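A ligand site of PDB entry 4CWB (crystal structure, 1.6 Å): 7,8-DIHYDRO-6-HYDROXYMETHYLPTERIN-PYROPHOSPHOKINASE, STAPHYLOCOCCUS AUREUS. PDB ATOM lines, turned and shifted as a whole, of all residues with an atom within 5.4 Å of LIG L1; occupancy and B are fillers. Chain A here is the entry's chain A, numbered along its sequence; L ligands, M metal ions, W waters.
N2 of LIG L1 sits at hydrogen-bond distance from N of Val 49, 2.9 Å away. The backbone carbonyl oxygen (O) of Val 49 sits at hydrogen-bond distance from a nitrogen (N3) of LIG L1 (2.9 Å). The side-chain hydroxyl (OG1) of Thr 46 is in hydrogen-bond range of a nitrogen (N5) of LIG L1 (2.9 Å). The backbone carbonyl oxygen of Ala 47 sits at hydrogen-bond distance from a nitrogen (N5) of LIG L1 (2.9 Å). An oxygen (O1) of LIG L1 is in hydrogen-bond range of the side-chain amide nitrogen of Asn 59, at 3.0 Å. The guanidinium group (NH2) of Arg 124 sits at hydrogen-bond distance from an oxygen (O2) of LIG L1, at 3.2 Å. A sulfur (S1) of LIG L1 sits close to the guanidinium group (NH2) of Arg 95 (3.6 Å). The guanidinium group (NH2) of Arg 124 lies within salt-bridge range of an oxygen (O1) of LG2 L2. The guanidinium group (NH1) of Arg 95 is in salt-bridge range of an oxygen (O5) of LG2 L2.
OG1 of Thr 46 lies within hydrogen-bond range of OD1 of Asn 59, 2.8 Å away. O of Thr 46 is in hydrogen-bond range of N of Phe 57. The backbone carbonyl oxygen of Arg 91 is in hydrogen-bond range of the guanidinium group of Arg 95, at 2.9 Å. O of Gly 93 lies within hydrogen-bond range of NE of Arg 95, at 2.9 Å. The guanidinium group of Arg 95 sits close to the side-chain carboxylate of Asp 98 (3.6 Å). The backbone carbonyl oxygen of Trp 92 is in hydrogen-bond range of the side-chain amide nitrogen of Gln 54 (3.1 Å).
A sulfur (S1) of LIG L1 lies close to the backbone carbonyl oxygen (O) of Arg 91, 3.7 Å away. O of Trp 92 sits close to S1 of LIG L1 (3.7 Å). Merely in contact with LIG L1: Phe 57 (3.3 Å), Phe 126 (3.4 Å), Pro 48 (3.6 Å) and Gly 50 (3.8 Å). Hydrophobic or aromatic side chains that line LIG L1: Val 49, Phe 57 and Phe 126. Within 4 Å of LIG L1: Thr 46, Ala 47, Pro 48, Val 49, Gly 50, Phe 57, Asn 59, Arg 91, Trp 92, Arg 95, Arg 124 and Phe 126. The nearest printed residue that does not touch LIG L1 is Gly 12 (4.4 Å).
Water W4 lies within hydrogen-bond range of an oxygen (O2) of LIG L1 (2.7 Å), an oxygen (O5) of LG2 L2 (3.5 Å) and the guanidinium group of Arg 95 (3.5 Å). Water W5 lies within hydrogen-bond range of O1 of LIG L1 (2.7 Å) and NH1 of Arg 95 (3.0 Å). Water W1 bridges the backbone carbonyl oxygen (O) of Arg 91 (2.9 Å) and an oxygen (O6) of LG2 L2 (3.1 Å).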
ATOM      1  N   GLY A  12      31.348  -9.261  -0.636  1.00  0.00           N
ATOM      2  CA  GLY A  12      31.082 -10.390   0.242  1.00  0.00           C
ATOM      3  C   GLY A  12      32.204 -11.394   0.168  1.00  0.00           C
ATOM      4  O   GLY A  12      32.842 -11.536  -0.859  1.00  0.00           O
ATOM      5  N   THR A  46      27.213 -12.180   8.613  1.00  0.00           N
ATOM      6  CA  THR A  46      25.893 -12.500   8.161  1.00  0.00           C
ATOM      7  C   THR A  46      25.773 -14.003   7.929  1.00  0.00           C
ATOM      8  O   THR A  46      26.667 -14.640   7.373  1.00  0.00           O
ATOM      9  CB  THR A  46      25.561 -11.704   6.864  1.00  0.00           C
ATOM     10  OG1 THR A  46      26.445 -12.062   5.826  1.00  0.00           O
ATOM     11  CG2 THR A  46      25.781 -10.192   7.074  1.00  0.00           C
ATOM     12  N   ALA A  47      24.679 -14.588   8.387  1.00  0.00           N
ATOM     13  CA  ALA A  47      24.407 -15.994   8.125  1.00  0.00           C
ATOM     14  C   ALA A  47      24.182 -16.191   6.606  1.00  0.00           C
ATOM     15  O   ALA A  47      23.617 -15.307   5.961  1.00  0.00           O
ATOM     16  CB  ALA A  47      23.168 -16.440   8.904  1.00  0.00           C
ATOM     17  N   PRO A  48      24.635 -17.318   6.032  1.00  0.00           N
ATOM     18  CA  PRO A  48      24.489 -17.492   4.593  1.00  0.00           C
ATOM     19  C   PRO A  48      23.020 -17.563   4.176  1.00  0.00           C
ATOM     20  O   PRO A  48      22.232 -18.239   4.837  1.00  0.00           O
ATOM     21  CB  PRO A  48      25.192 -18.826   4.316  1.00  0.00           C
ATOM     22  CG  PRO A  48      25.173 -19.544   5.614  1.00  0.00           C
ATOM     23  CD  PRO A  48      25.258 -18.501   6.667  1.00  0.00           C
ATOM     24  N   VAL A  49      22.702 -16.867   3.102  1.00  0.00           N
ATOM     25  CA  VAL A  49      21.371 -16.858   2.525  1.00  0.00           C
ATOM     26  C   VAL A  49      21.337 -17.719   1.279  1.00  0.00           C
ATOM     27  O   VAL A  49      22.216 -17.649   0.430  1.00  0.00           O
ATOM     28  CB  VAL A  49      20.931 -15.444   2.203  1.00  0.00           C
ATOM     29  CG1 VAL A  49      19.505 -15.451   1.699  1.00  0.00           C
ATOM     30  CG2 VAL A  49      21.014 -14.548   3.435  1.00  0.00           C
ATOM     31  N   GLY A  50      20.278 -18.519   1.187  1.00  0.00           N
ATOM     32  CA  GLY A  50      20.084 -19.469   0.078  1.00  0.00           C
ATOM     33  C   GLY A  50      20.461 -20.860   0.499  1.00  0.00           C
ATOM     34  O   GLY A  50      19.755 -21.478   1.293  1.00  0.00           O
ATOM     35  N   TYR A  51      21.605 -21.340   0.014  1.00  0.00           N
ATOM     36  CA  TYR A  51      22.186 -22.601   0.464  1.00  0.00           C
ATOM     37  C   TYR A  51      22.871 -22.342   1.813  1.00  0.00           C
ATOM     38  O   TYR A  51      23.706 -21.454   1.900  1.00  0.00           O
ATOM     39  CB  TYR A  51      23.205 -23.074  -0.570  1.00  0.00           C
ATOM     40  CG  TYR A  51      24.010 -24.316  -0.228  1.00  0.00           C
ATOM     41  CD1 TYR A  51      23.403 -25.552  -0.118  1.00  0.00           C
ATOM     42  CD2 TYR A  51      25.379 -24.227  -0.058  1.00  0.00           C
ATOM     43  CE1 TYR A  51      24.155 -26.681   0.187  1.00  0.00           C
ATOM     44  CE2 TYR A  51      26.132 -25.342   0.221  1.00  0.00           C
ATOM     45  CZ  TYR A  51      25.516 -26.559   0.341  1.00  0.00           C
ATOM     46  OH  TYR A  51      26.317 -27.653   0.632  1.00  0.00           O
ATOM     47  N   GLN A  54      27.152 -23.708   4.197  1.00  0.00           N
ATOM     48  CA  GLN A  54      28.353 -23.028   3.757  1.00  0.00           C
ATOM     49  C   GLN A  54      28.686 -21.957   4.789  1.00  0.00           C
ATOM     50  O   GLN A  54      27.865 -21.672   5.656  1.00  0.00           O
ATOM     51  CB  GLN A  54      28.150 -22.422   2.367  1.00  0.00           C
ATOM     52  CG  GLN A  54      27.196 -21.251   2.330  1.00  0.00           C
ATOM     53  CD  GLN A  54      27.160 -20.629   0.965  1.00  0.00           C
ATOM     54  OE1 GLN A  54      28.175 -20.293   0.368  1.00  0.00           O
ATOM     55  NE2 GLN A  54      25.945 -20.439   0.448  1.00  0.00           N
ATOM     56  N   PHE A  57      29.157 -15.237   6.128  1.00  0.00           N
ATOM     57  CA  PHE A  57      29.745 -14.214   5.285  1.00  0.00           C
ATOM     58  C   PHE A  57      30.176 -12.994   6.079  1.00  0.00           C
ATOM     59  O   PHE A  57      29.586 -12.706   7.100  1.00  0.00           O
ATOM     60  CB  PHE A  57      28.704 -13.722   4.269  1.00  0.00           C
ATOM     61  CG  PHE A  57      28.520 -14.631   3.087  1.00  0.00           C
ATOM     62  CD1 PHE A  57      27.729 -15.768   3.210  1.00  0.00           C
ATOM     63  CD2 PHE A  57      29.110 -14.357   1.882  1.00  0.00           C
ATOM     64  CE1 PHE A  57      27.550 -16.610   2.125  1.00  0.00           C
ATOM     65  CE2 PHE A  57      28.961 -15.217   0.795  1.00  0.00           C
ATOM     66  CZ  PHE A  57      28.162 -16.336   0.927  1.00  0.00           C
ATOM     67  N   ASN A  59      30.146  -9.080   4.901  1.00  0.00           N
ATOM     68  CA  ASN A  59      29.613  -8.218   3.847  1.00  0.00           C
ATOM     69  C   ASN A  59      29.857  -6.752   4.180  1.00  0.00           C
ATOM     70  O   ASN A  59      29.842  -6.349   5.352  1.00  0.00           O
ATOM     71  CB  ASN A  59      28.106  -8.412   3.712  1.00  0.00           C
ATOM     72  CG  ASN A  59      27.739  -9.699   2.990  1.00  0.00           C
ATOM     73  OD1 ASN A  59      27.138 -10.605   3.570  1.00  0.00           O
ATOM     74  ND2 ASN A  59      28.032  -9.746   1.704  1.00  0.00           N
ATOM     75  N   ARG A  91      26.810 -20.177  -8.432  1.00  0.00           N
ATOM     76  CA  ARG A  91      26.250 -18.918  -7.980  1.00  0.00           C
ATOM     77  C   ARG A  91      25.683 -19.024  -6.592  1.00  0.00           C
ATOM     78  O   ARG A  91      25.613 -18.035  -5.876  1.00  0.00           O
ATOM     79  CB  ARG A  91      25.122 -18.474  -8.907  1.00  0.00           C
ATOM     80  CG  ARG A  91      25.545 -18.043 -10.299  1.00  0.00           C
ATOM     81  CD  ARG A  91      24.278 -17.678 -11.080  1.00  0.00           C
ATOM     82  NE  ARG A  91      23.482 -16.638 -10.391  1.00  0.00           N
ATOM     83  CZ  ARG A  91      23.320 -15.394 -10.831  1.00  0.00           C
ATOM     84  NH1 ARG A  91      23.885 -14.980 -11.961  1.00  0.00           N
ATOM     85  NH2 ARG A  91      22.583 -14.534 -10.129  1.00  0.00           N
ATOM     86  N   TRP A  92      25.271 -20.217  -6.194  1.00  0.00           N
ATOM     87  CA  TRP A  92      24.650 -20.423  -4.902  1.00  0.00           C
ATOM     88  C   TRP A  92      25.652 -20.690  -3.777  1.00  0.00           C
ATOM     89  O   TRP A  92      25.288 -20.673  -2.605  1.00  0.00           O
ATOM     90  CB  TRP A  92      23.623 -21.578  -4.971  1.00  0.00           C
ATOM     91  CG  TRP A  92      24.148 -22.827  -5.581  1.00  0.00           C
ATOM     92  CD1 TRP A  92      23.978 -23.247  -6.856  1.00  0.00           C
ATOM     93  CD2 TRP A  92      24.960 -23.828  -4.940  1.00  0.00           C
ATOM     94  NE1 TRP A  92      24.606 -24.446  -7.053  1.00  0.00           N
ATOM     95  CE2 TRP A  92      25.222 -24.822  -5.898  1.00  0.00           C
ATOM     96  CE3 TRP A  92      25.479 -23.975  -3.649  1.00  0.00           C
ATOM     97  CZ2 TRP A  92      25.982 -25.960  -5.601  1.00  0.00           C
ATOM     98  CZ3 TRP A  92      26.231 -25.093  -3.357  1.00  0.00           C
ATOM     99  CH2 TRP A  92      26.491 -26.055  -4.324  1.00  0.00           C
ATOM    100  N   GLY A  93      26.880 -20.976  -4.173  1.00  0.00           N
ATOM    101  CA  GLY A  93      27.888 -21.526  -3.266  1.00  0.00           C
ATOM    102  C   GLY A  93      28.922 -20.529  -2.783  1.00  0.00           C
ATOM    103  O   GLY A  93      28.890 -19.334  -3.102  1.00  0.00           O
ATOM    104  N   ARG A  95      32.396 -18.402  -1.866  1.00  0.00           N
ATOM    105  CA  ARG A  95      33.330 -17.646  -2.680  1.00  0.00           C
ATOM    106  C   ARG A  95      34.281 -16.831  -1.797  1.00  0.00           C
ATOM    107  O   ARG A  95      33.897 -16.289  -0.766  1.00  0.00           O
ATOM    108  CB  ARG A  95      32.629 -16.726  -3.713  1.00  0.00           C
ATOM    109  CG  ARG A  95      31.916 -15.478  -3.177  1.00  0.00           C
ATOM    110  CD  ARG A  95      30.645 -15.737  -2.380  1.00  0.00           C
ATOM    111  NE  ARG A  95      29.701 -16.585  -3.096  1.00  0.00           N
ATOM    112  CZ  ARG A  95      28.798 -16.154  -3.971  1.00  0.00           C
ATOM    113  NH1 ARG A  95      28.620 -14.850  -4.189  1.00  0.00           N
ATOM    114  NH2 ARG A  95      28.051 -17.039  -4.626  1.00  0.00           N
ATOM    115  N   ASP A  98      33.038 -11.748  -3.696  1.00  0.00           N
ATOM    116  CA  ASP A  98      31.960 -11.355  -4.593  1.00  0.00           C
ATOM    117  C   ASP A  98      31.930  -9.827  -4.614  1.00  0.00           C
ATOM    118  O   ASP A  98      31.916  -9.195  -3.560  1.00  0.00           O
ATOM    119  CB  ASP A  98      30.632 -11.885  -4.052  1.00  0.00           C
ATOM    120  CG  ASP A  98      29.459 -11.569  -4.950  1.00  0.00           C
ATOM    121  OD1 ASP A  98      29.617 -11.673  -6.172  1.00  0.00           O
ATOM    122  OD2 ASP A  98      28.357 -11.287  -4.397  1.00  0.00           O
ATOM    123  N   ARG A 124      17.565  -7.832   0.754  1.00  0.00           N
ATOM    124  CA  ARG A 124      18.749  -8.390   1.432  1.00  0.00           C
ATOM    125  C   ARG A 124      19.258  -7.465   2.495  1.00  0.00           C
ATOM    126  O   ARG A 124      19.836  -6.417   2.192  1.00  0.00           O
ATOM    127  CB  ARG A 124      19.860  -8.672   0.452  1.00  0.00           C
ATOM    128  CG  ARG A 124      19.540  -9.744  -0.566  1.00  0.00           C
ATOM    129  CD  ARG A 124      20.560  -9.761  -1.671  1.00  0.00           C
ATOM    130  NE  ARG A 124      20.442 -10.958  -2.504  1.00  0.00           N
ATOM    131  CZ  ARG A 124      21.307 -11.299  -3.455  1.00  0.00           C
ATOM    132  NH1 ARG A 124      22.381 -10.548  -3.734  1.00  0.00           N
ATOM    133  NH2 ARG A 124      21.071 -12.376  -4.183  1.00  0.00           N
ATOM    134  N   PHE A 126      21.815  -8.041   4.266  1.00  0.00           N
ATOM    135  CA  PHE A 126      23.282  -8.071   4.174  1.00  0.00           C
ATOM    136  C   PHE A 126      23.814  -7.029   3.167  1.00  0.00           C
ATOM    137  O   PHE A 126      25.011  -6.711   3.148  1.00  0.00           O
ATOM    138  CB  PHE A 126      23.832  -9.479   3.922  1.00  0.00           C
ATOM    139  CG  PHE A 126      23.592 -10.060   2.535  1.00  0.00           C
ATOM    140  CD1 PHE A 126      24.373  -9.663   1.477  1.00  0.00           C
ATOM    141  CD2 PHE A 126      22.657 -11.080   2.339  1.00  0.00           C
ATOM    142  CE1 PHE A 126      24.233 -10.245   0.215  1.00  0.00           C
ATOM    143  CE2 PHE A 126      22.516 -11.674   1.090  1.00  0.00           C
ATOM    144  CZ  PHE A 126      23.296 -11.248   0.036  1.00  0.00           C
HETATM  145  C1  LIG L   1      15.541 -18.063  -2.349  1.00  0.00           C
HETATM  146  C2  LIG L   1      16.077 -17.390  -1.277  1.00  0.00           C
HETATM  147  C3  LIG L   1      16.330 -18.299  -3.438  1.00  0.00           C
HETATM  148  C4  LIG L   1      17.383 -16.961  -1.319  1.00  0.00           C
HETATM  149  C5  LIG L   1      17.642 -17.871  -3.473  1.00  0.00           C
HETATM  150  C6  LIG L   1      20.526 -17.383  -3.252  1.00  0.00           C
HETATM  151  C7  LIG L   1      19.936 -15.482  -1.974  1.00  0.00           C
HETATM  152  C8  LIG L   1      21.784 -16.856  -3.432  1.00  0.00           C
HETATM  153  C9  LIG L   1      21.188 -14.945  -2.161  1.00  0.00           C
HETATM  154  C10 LIG L   1      18.193 -17.197  -2.400  1.00  0.00           C
HETATM  155  C11 LIG L   1      19.564 -16.713  -2.524  1.00  0.00           C
HETATM  156  C12 LIG L   1      22.116 -15.636  -2.901  1.00  0.00           C
HETATM  157  C13 LIG L   1      25.780 -14.156   0.214  1.00  0.00           C
HETATM  158  C14 LIG L   1      24.946 -14.942   0.921  1.00  0.00           C
HETATM  159  C15 LIG L   1      25.334 -15.777  -1.059  1.00  0.00           C
HETATM  160  C16 LIG L   1      26.278 -12.958   0.837  1.00  0.00           C
HETATM  161  C17 LIG L   1      24.953 -13.737   2.737  1.00  0.00           C
HETATM  162  C18 LIG L   1      23.451 -15.037  -3.131  1.00  0.00           C
HETATM  163  C19 LIG L   1      24.619 -15.831  -3.610  1.00  0.00           C
HETATM  164  N1  LIG L   1      26.026 -14.665  -1.040  1.00  0.00           N
HETATM  165  N2  LIG L   1      24.488 -14.808   2.163  1.00  0.00           N
HETATM  166  N3  LIG L   1      24.629 -15.989   0.093  1.00  0.00           N
HETATM  167  N4  LIG L   1      25.804 -12.843   2.132  1.00  0.00           N
HETATM  168  N5  LIG L   1      24.639 -13.405   3.998  1.00  0.00           N
HETATM  169  O1  LIG L   1      27.044 -12.164   0.328  1.00  0.00           O
HETATM  170  O2  LIG L   1      23.606 -13.859  -2.957  1.00  0.00           O
HETATM  171  S1  LIG L   1      25.226 -16.938  -2.358  1.00  0.00           S
HETATM  172  P1  LG2 L   2      23.905 -11.986  -6.703  1.00  0.00           P
HETATM  173  O1  LG2 L   2      22.390 -12.261  -6.621  1.00  0.00           O
HETATM  174  O2  LG2 L   2      24.318 -11.250  -7.966  1.00  0.00           O
HETATM  175  O3  LG2 L   2      24.407 -11.414  -5.433  1.00  0.00           O
HETATM  176  P2  LG2 L   2      26.119 -13.713  -6.992  1.00  0.00           P
HETATM  177  O4  LG2 L   2      26.852 -12.438  -6.605  1.00  0.00           O
HETATM  178  O5  LG2 L   2      26.490 -14.970  -6.080  1.00  0.00           O
HETATM  179  O6  LG2 L   2      24.542 -13.460  -6.810  1.00  0.00           O
HETATM  180  P3  LG2 L   2      27.971 -14.103  -9.347  1.00  0.00           P
HETATM  181  O7  LG2 L   2      28.843 -13.155  -8.585  1.00  0.00           O
HETATM  182  O8  LG2 L   2      28.405 -15.636  -9.193  1.00  0.00           O
HETATM  183  C1  LG2 L   2      26.288 -14.004  -8.755  1.00  0.00           C
HETATM  184  O9  LG2 L   2      28.027 -13.479 -10.836  1.00  0.00           O
HETATM  185  C2  LG2 L   2      27.432 -14.068 -11.956  1.00  0.00           C
HETATM  186  C3  LG2 L   2      26.980 -12.971 -12.916  1.00  0.00           C
HETATM  187  O10 LG2 L   2      25.960 -12.156 -12.313  1.00  0.00           O
HETATM  188  C4  LG2 L   2      27.995 -11.952 -13.403  1.00  0.00           C
HETATM  189  O11 LG2 L   2      28.987 -12.452 -14.320  1.00  0.00           O
HETATM  190  C5  LG2 L   2      27.036 -10.968 -14.060  1.00  0.00           C
HETATM  191  O12 LG2 L   2      26.825 -11.293 -15.453  1.00  0.00           O
HETATM  192  C6  LG2 L   2      25.736 -11.173 -13.300  1.00  0.00           C
HETATM  193  N1  LG2 L   2      25.214  -9.902 -12.773  1.00  0.00           N
HETATM  194  C7  LG2 L   2      24.014  -9.391 -13.115  1.00  0.00           C
HETATM  195  N2  LG2 L   2      23.799  -8.200 -12.535  1.00  0.00           N
HETATM  196  C8  LG2 L   2      24.928  -7.929 -11.807  1.00  0.00           C
HETATM  197  C9  LG2 L   2      25.353  -6.821 -10.936  1.00  0.00           C
HETATM  198  N3  LG2 L   2      24.548  -5.756 -10.724  1.00  0.00           N
HETATM  199  N4  LG2 L   2      26.571  -6.954 -10.389  1.00  0.00           N
HETATM  200  C10 LG2 L   2      27.389  -8.000 -10.584  1.00  0.00           C
HETATM  201  N5  LG2 L   2      27.047  -9.047 -11.349  1.00  0.00           N
HETATM  202  C11 LG2 L   2      25.855  -9.044 -11.970  1.00  0.00           C
HETATM  203 MG    MG M   1      26.363 -11.293  -5.008  1.00  0.00          MG
HETATM  204  O   HOH W   1      23.513 -16.361  -6.833  1.00  0.00           O
HETATM  205  O   HOH W   2      22.939 -19.649  -1.749  1.00  0.00           O
HETATM  206  O   HOH W   3      19.579 -15.132  -5.602  1.00  0.00           O
HETATM  207  O   HOH W   4      25.986 -12.640  -3.558  1.00  0.00           O
HETATM  208  O   HOH W   5      28.484 -12.944  -1.873  1.00  0.00           O
